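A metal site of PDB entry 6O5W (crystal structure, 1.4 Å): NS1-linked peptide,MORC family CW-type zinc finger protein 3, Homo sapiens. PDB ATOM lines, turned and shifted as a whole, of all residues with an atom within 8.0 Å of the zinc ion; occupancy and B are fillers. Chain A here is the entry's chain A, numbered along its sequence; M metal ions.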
ATOM      1  N   GLN A  16     -25.857  -2.184 -25.795  1.00  0.00           N
ATOM      2  CA  GLN A  16     -26.964  -3.142 -25.789  1.00  0.00           C
ATOM      3  C   GLN A  16     -27.176  -3.732 -27.173  1.00  0.00           C
ATOM      4  O   GLN A  16     -27.210  -3.001 -28.165  1.00  0.00           O
ATOM      5  CB  GLN A  16     -28.259  -2.486 -25.320  1.00  0.00           C
ATOM      6  CG  GLN A  16     -29.281  -3.512 -24.910  1.00  0.00           C
ATOM      7  CD  GLN A  16     -30.579  -2.895 -24.478  1.00  0.00           C
ATOM      8  OE1 GLN A  16     -30.966  -1.810 -24.925  1.00  0.00           O
ATOM      9  NE2 GLN A  16     -31.223  -3.540 -23.522  1.00  0.00           N
ATOM     10  N   CYS A  17     -27.344  -5.052 -27.215  1.00  0.00           N
ATOM     11  CA  CYS A  17     -27.708  -5.691 -28.472  1.00  0.00           C
ATOM     12  C   CYS A  17     -29.149  -5.354 -28.821  1.00  0.00           C
ATOM     13  O   CYS A  17     -30.073  -5.577 -28.028  1.00  0.00           O
ATOM     14  CB  CYS A  17     -27.554  -7.202 -28.335  1.00  0.00           C
ATOM     15  SG  CYS A  17     -28.085  -8.104 -29.810  1.00  0.00           S
ATOM     16  N   ASP A  18     -29.345  -4.860 -30.044  1.00  0.00           N
ATOM     17  CA  ASP A  18     -30.677  -4.456 -30.492  1.00  0.00           C
ATOM     18  C   ASP A  18     -31.581  -5.648 -30.748  1.00  0.00           C
ATOM     19  O   ASP A  18     -32.804  -5.458 -30.877  1.00  0.00           O
ATOM     20  CB  ASP A  18     -30.511  -3.609 -31.749  1.00  0.00           C
ATOM     21  CG  ASP A  18     -30.385  -2.155 -31.435  1.00  0.00           C
ATOM     22  OD1 ASP A  18     -31.361  -1.577 -30.908  1.00  0.00           O
ATOM     23  OD2 ASP A  18     -29.274  -1.611 -31.595  1.00  0.00           O
ATOM     24  N   ALA A  19     -31.043  -6.864 -30.807  1.00  0.00           N
ATOM     25  CA  ALA A  19     -31.842  -8.065 -30.993  1.00  0.00           C
ATOM     26  C   ALA A  19     -32.223  -8.751 -29.686  1.00  0.00           C
ATOM     27  O   ALA A  19     -33.392  -9.073 -29.469  1.00  0.00           O
ATOM     28  CB  ALA A  19     -31.136  -9.046 -31.924  1.00  0.00           C
ATOM     29  N   CYS A  20     -31.258  -9.007 -28.806  1.00  0.00           N
ATOM     30  CA  CYS A  20     -31.516  -9.799 -27.604  1.00  0.00           C
ATOM     31  C   CYS A  20     -31.538  -8.961 -26.342  1.00  0.00           C
ATOM     32  O   CYS A  20     -31.847  -9.488 -25.265  1.00  0.00           O
ATOM     33  CB  CYS A  20     -30.483 -10.930 -27.449  1.00  0.00           C
ATOM     34  SG  CYS A  20     -28.843 -10.377 -26.905  1.00  0.00           S
ATOM     35  N   LEU A  21     -31.199  -7.675 -26.431  1.00  0.00           N
ATOM     36  CA  LEU A  21     -31.214  -6.717 -25.332  1.00  0.00           C
ATOM     37  C   LEU A  21     -30.157  -6.981 -24.257  1.00  0.00           C
ATOM     38  O   LEU A  21     -30.149  -6.279 -23.232  1.00  0.00           O
ATOM     39  CB  LEU A  21     -32.599  -6.504 -24.720  1.00  0.00           C
ATOM     40  CG  LEU A  21     -33.643  -6.028 -25.715  1.00  0.00           C
ATOM     41  CD1 LEU A  21     -34.964  -5.793 -24.998  1.00  0.00           C
ATOM     42  CD2 LEU A  21     -33.211  -4.772 -26.444  1.00  0.00           C
ATOM     43  N   LYS A  22     -29.289  -7.968 -24.436  1.00  0.00           N
ATOM     44  CA  LYS A  22     -28.191  -8.141 -23.499  1.00  0.00           C
ATOM     45  C   LYS A  22     -27.192  -7.006 -23.640  1.00  0.00           C
ATOM     46  O   LYS A  22     -27.037  -6.402 -24.705  1.00  0.00           O
ATOM     47  CB  LYS A  22     -27.471  -9.461 -23.752  1.00  0.00           C
ATOM     48  CG  LYS A  22     -28.263 -10.687 -23.355  1.00  0.00           C
ATOM     49  CD  LYS A  22     -27.415 -11.933 -23.543  1.00  0.00           C
ATOM     50  CE  LYS A  22     -28.180 -13.198 -23.234  1.00  0.00           C
ATOM     51  NZ  LYS A  22     -29.211 -13.507 -24.267  1.00  0.00           N
ATOM     52  N   TRP A  23     -26.516  -6.714 -22.540  1.00  0.00           N
ATOM     53  CA  TRP A  23     -25.491  -5.676 -22.506  1.00  0.00           C
ATOM     54  C   TRP A  23     -24.116  -6.304 -22.663  1.00  0.00           C
ATOM     55  O   TRP A  23     -23.793  -7.275 -21.968  1.00  0.00           O
ATOM     56  CB  TRP A  23     -25.596  -4.932 -21.184  1.00  0.00           C
ATOM     57  CG  TRP A  23     -26.884  -4.166 -21.080  1.00  0.00           C
ATOM     58  CD1 TRP A  23     -28.075  -4.632 -20.585  1.00  0.00           C
ATOM     59  CD2 TRP A  23     -27.114  -2.830 -21.521  1.00  0.00           C
ATOM     60  NE1 TRP A  23     -29.024  -3.644 -20.672  1.00  0.00           N
ATOM     61  CE2 TRP A  23     -28.461  -2.532 -21.237  1.00  0.00           C
ATOM     62  CE3 TRP A  23     -26.311  -1.835 -22.101  1.00  0.00           C
ATOM     63  CZ2 TRP A  23     -29.031  -1.288 -21.534  1.00  0.00           C
ATOM     64  CZ3 TRP A  23     -26.880  -0.608 -22.394  1.00  0.00           C
ATOM     65  CH2 TRP A  23     -28.227  -0.344 -22.101  1.00  0.00           C
ATOM     66  N   ARG A  24     -23.330  -5.773 -23.588  1.00  0.00           N
ATOM     67  CA  ARG A  24     -21.985  -6.275 -23.853  1.00  0.00           C
ATOM     68  C   ARG A  24     -20.965  -5.199 -23.527  1.00  0.00           C
ATOM     69  O   ARG A  24     -21.205  -4.013 -23.783  1.00  0.00           O
ATOM     70  CB  ARG A  24     -21.833  -6.681 -25.328  1.00  0.00           C
ATOM     71  CG  ARG A  24     -22.861  -7.701 -25.806  1.00  0.00           C
ATOM     72  CD  ARG A  24     -22.830  -8.949 -24.953  1.00  0.00           C
ATOM     73  NE  ARG A  24     -23.620 -10.023 -25.553  1.00  0.00           N
ATOM     74  CZ  ARG A  24     -23.906 -11.160 -24.932  1.00  0.00           C
ATOM     75  NH1 ARG A  24     -23.493 -11.383 -23.698  1.00  0.00           N
ATOM     76  NH2 ARG A  24     -24.600 -12.093 -25.577  1.00  0.00           N
ATOM     77  N   TRP A  37     -26.716  -1.983 -33.001  1.00  0.00           N
ATOM     78  CA  TRP A  37     -25.564  -2.821 -32.649  1.00  0.00           C
ATOM     79  C   TRP A  37     -26.083  -4.179 -32.193  1.00  0.00           C
ATOM     80  O   TRP A  37     -27.086  -4.251 -31.475  1.00  0.00           O
ATOM     81  CB  TRP A  37     -24.737  -2.179 -31.524  1.00  0.00           C
ATOM     82  CG  TRP A  37     -23.431  -2.862 -31.279  1.00  0.00           C
ATOM     83  CD1 TRP A  37     -22.239  -2.560 -31.862  1.00  0.00           C
ATOM     84  CD2 TRP A  37     -23.187  -3.976 -30.412  1.00  0.00           C
ATOM     85  NE1 TRP A  37     -21.255  -3.411 -31.398  1.00  0.00           N
ATOM     86  CE2 TRP A  37     -21.815  -4.291 -30.511  1.00  0.00           C
ATOM     87  CE3 TRP A  37     -23.999  -4.735 -29.560  1.00  0.00           C
ATOM     88  CZ2 TRP A  37     -21.232  -5.330 -29.784  1.00  0.00           C
ATOM     89  CZ3 TRP A  37     -23.412  -5.777 -28.846  1.00  0.00           C
ATOM     90  CH2 TRP A  37     -22.049  -6.065 -28.954  1.00  0.00           C
ATOM     91  N   TYR A  38     -25.407  -5.237 -32.629  1.00  0.00           N
ATOM     92  CA  TYR A  38     -25.812  -6.594 -32.299  1.00  0.00           C
ATOM     93  C   TYR A  38     -24.618  -7.361 -31.764  1.00  0.00           C
ATOM     94  O   TYR A  38     -23.468  -7.024 -32.058  1.00  0.00           O
ATOM     95  CB  TYR A  38     -26.349  -7.340 -33.535  1.00  0.00           C
ATOM     96  CG  TYR A  38     -27.514  -6.616 -34.149  1.00  0.00           C
ATOM     97  CD1 TYR A  38     -28.782  -6.757 -33.628  1.00  0.00           C
ATOM     98  CD2 TYR A  38     -27.346  -5.789 -35.250  1.00  0.00           C
ATOM     99  CE1 TYR A  38     -29.856  -6.088 -34.164  1.00  0.00           C
ATOM    100  CE2 TYR A  38     -28.425  -5.113 -35.805  1.00  0.00           C
ATOM    101  CZ  TYR A  38     -29.677  -5.275 -35.251  1.00  0.00           C
ATOM    102  OH  TYR A  38     -30.779  -4.622 -35.777  1.00  0.00           O
ATOM    103  N   CYS A  39     -24.895  -8.402 -30.975  1.00  0.00           N
ATOM    104  CA  CYS A  39     -23.818  -9.270 -30.517  1.00  0.00           C
ATOM    105  C   CYS A  39     -22.963  -9.711 -31.689  1.00  0.00           C
ATOM    106  O   CYS A  39     -21.736  -9.794 -31.584  1.00  0.00           O
ATOM    107  CB  CYS A  39     -24.402 -10.496 -29.817  1.00  0.00           C
ATOM    108  SG  CYS A  39     -25.343 -10.127 -28.312  1.00  0.00           S
ATOM    109  N   SER A  40     -23.599  -9.967 -32.839  1.00  0.00           N
ATOM    110  CA  SER A  40     -22.864 -10.420 -34.020  1.00  0.00           C
ATOM    111  C   SER A  40     -21.799  -9.425 -34.486  1.00  0.00           C
ATOM    112  O   SER A  40     -20.878  -9.837 -35.199  1.00  0.00           O
ATOM    113  CB  SER A  40     -23.851 -10.759 -35.131  1.00  0.00           C
ATOM    114  OG  SER A  40     -24.752  -9.690 -35.330  1.00  0.00           O
ATOM    115  N   PHE A  47     -18.350 -13.015 -27.222  1.00  0.00           N
ATOM    116  CA  PHE A  47     -19.603 -12.327 -26.937  1.00  0.00           C
ATOM    117  C   PHE A  47     -20.277 -11.892 -28.224  1.00  0.00           C
ATOM    118  O   PHE A  47     -20.814 -10.786 -28.341  1.00  0.00           O
ATOM    119  CB  PHE A  47     -19.390 -11.159 -25.975  1.00  0.00           C
ATOM    120  CG  PHE A  47     -18.872 -11.599 -24.642  1.00  0.00           C
ATOM    121  CD1 PHE A  47     -19.729 -12.154 -23.710  1.00  0.00           C
ATOM    122  CD2 PHE A  47     -17.530 -11.510 -24.343  1.00  0.00           C
ATOM    123  CE1 PHE A  47     -19.254 -12.593 -22.488  1.00  0.00           C
ATOM    124  CE2 PHE A  47     -17.051 -11.940 -23.107  1.00  0.00           C
ATOM    125  CZ  PHE A  47     -17.919 -12.481 -22.189  1.00  0.00           C
ATOM    126  N   ARG A  48     -20.281 -12.808 -29.202  1.00  0.00           N
ATOM    127  CA  ARG A  48     -20.711 -12.535 -30.567  1.00  0.00           C
ATOM    128  C   ARG A  48     -22.005 -13.245 -30.904  1.00  0.00           C
ATOM    129  O   ARG A  48     -22.533 -13.070 -32.008  1.00  0.00           O
ATOM    130  CB  ARG A  48     -19.569 -12.972 -31.497  1.00  0.00           C
ATOM    131  CG  ARG A  48     -19.745 -12.728 -32.978  1.00  0.00           C
ATOM    132  CD  ARG A  48     -18.459 -13.142 -33.690  1.00  0.00           C
ATOM    133  NE  ARG A  48     -17.409 -12.177 -33.404  1.00  0.00           N
ATOM    134  CZ  ARG A  48     -16.123 -12.352 -33.692  1.00  0.00           C
ATOM    135  NH1 ARG A  48     -15.690 -13.464 -34.268  1.00  0.00           N
ATOM    136  NH2 ARG A  48     -15.270 -11.385 -33.402  1.00  0.00           N
ATOM    137  N   ASN A  49     -22.566 -14.003 -29.979  1.00  0.00           N
ATOM    138  CA  ASN A  49     -23.825 -14.691 -30.183  1.00  0.00           C
ATOM    139  C   ASN A  49     -24.787 -14.271 -29.082  1.00  0.00           C
ATOM    140  O   ASN A  49     -24.394 -14.161 -27.921  1.00  0.00           O
ATOM    141  CB  ASN A  49     -23.624 -16.214 -30.173  1.00  0.00           C
ATOM    142  CG  ASN A  49     -24.844 -16.965 -30.675  1.00  0.00           C
ATOM    143  OD1 ASN A  49     -25.866 -17.025 -30.003  1.00  0.00           O
ATOM    144  ND2 ASN A  49     -24.738 -17.518 -31.877  1.00  0.00           N
ATOM    145  N   CYS A  50     -26.041 -14.031 -29.460  1.00  0.00           N
ATOM    146  CA  CYS A  50     -27.036 -13.587 -28.496  1.00  0.00           C
ATOM    147  C   CYS A  50     -27.243 -14.590 -27.379  1.00  0.00           C
ATOM    148  O   CYS A  50     -27.725 -14.212 -26.310  1.00  0.00           O
ATOM    149  CB  CYS A  50     -28.361 -13.305 -29.215  1.00  0.00           C
ATOM    150  SG  CYS A  50     -28.289 -11.873 -30.295  1.00  0.00           S
ATOM    151  N   GLU A  51     -26.895 -15.859 -27.578  1.00  0.00           N
ATOM    152  CA  GLU A  51     -27.092 -16.850 -26.536  1.00  0.00           C
ATOM    153  C   GLU A  51     -26.046 -16.787 -25.438  1.00  0.00           C
ATOM    154  O   GLU A  51     -26.271 -17.368 -24.370  1.00  0.00           O
ATOM    155  CB  GLU A  51     -27.125 -18.259 -27.152  1.00  0.00           C
ATOM    156  CG  GLU A  51     -28.234 -18.445 -28.162  1.00  0.00           C
ATOM    157  CD  GLU A  51     -29.599 -18.091 -27.608  1.00  0.00           C
ATOM    158  OE1 GLU A  51     -29.887 -18.447 -26.447  1.00  0.00           O
ATOM    159  OE2 GLU A  51     -30.385 -17.438 -28.330  1.00  0.00           O
ATOM    160  N   VAL A  52     -24.929 -16.103 -25.654  1.00  0.00           N
ATOM    161  CA  VAL A  52     -23.913 -16.031 -24.590  1.00  0.00           C
ATOM    162  C   VAL A  52     -24.470 -15.225 -23.422  1.00  0.00           C
ATOM    163  O   VAL A  52     -24.924 -14.084 -23.622  1.00  0.00           O
ATOM    164  CB  VAL A  52     -22.630 -15.404 -25.121  1.00  0.00           C
ATOM    165  CG1 VAL A  52     -21.620 -15.253 -23.980  1.00  0.00           C
ATOM    166  CG2 VAL A  52     -22.037 -16.243 -26.233  1.00  0.00           C
HETATM  167 ZN    ZN M   1     -27.628 -10.196 -28.852  1.00  0.00          ZN
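N of Lys 22 sits close to SG of Cys 20, 3.5 Å away.
The backbone carbonyl oxygen (O) of Cys 50 sits at hydrogen-bond distance from the side-chain amino group (NZ) of Lys 22 (2.6 Å).
The side-chain sulfur of Cys 17 lies close to the backbone NH of Ala 19 (3.4 Å).
The backbone carbonyl oxygen of Lys 22 sits at hydrogen-bond distance from the backbone NH of Cys 17, at 2.9 Å.
SG of Cys 39 lies close to NE of Arg 24, at 3.3 Å.
Of the 19 residues printed, 4 come within 4 Å of the zinc ion.
The nearest printed residue that does not touch the zinc ion is Ala 19 (4.8 Å).
The zinc ion is bound by SG of Cys 20 (2.3 Å), SG of Cys 50 (2.3 Å), SG of Cys 17 (2.3 Å) and SG of Cys 39 (2.3 Å).
The zinc ion has four donor atoms within binding distance.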
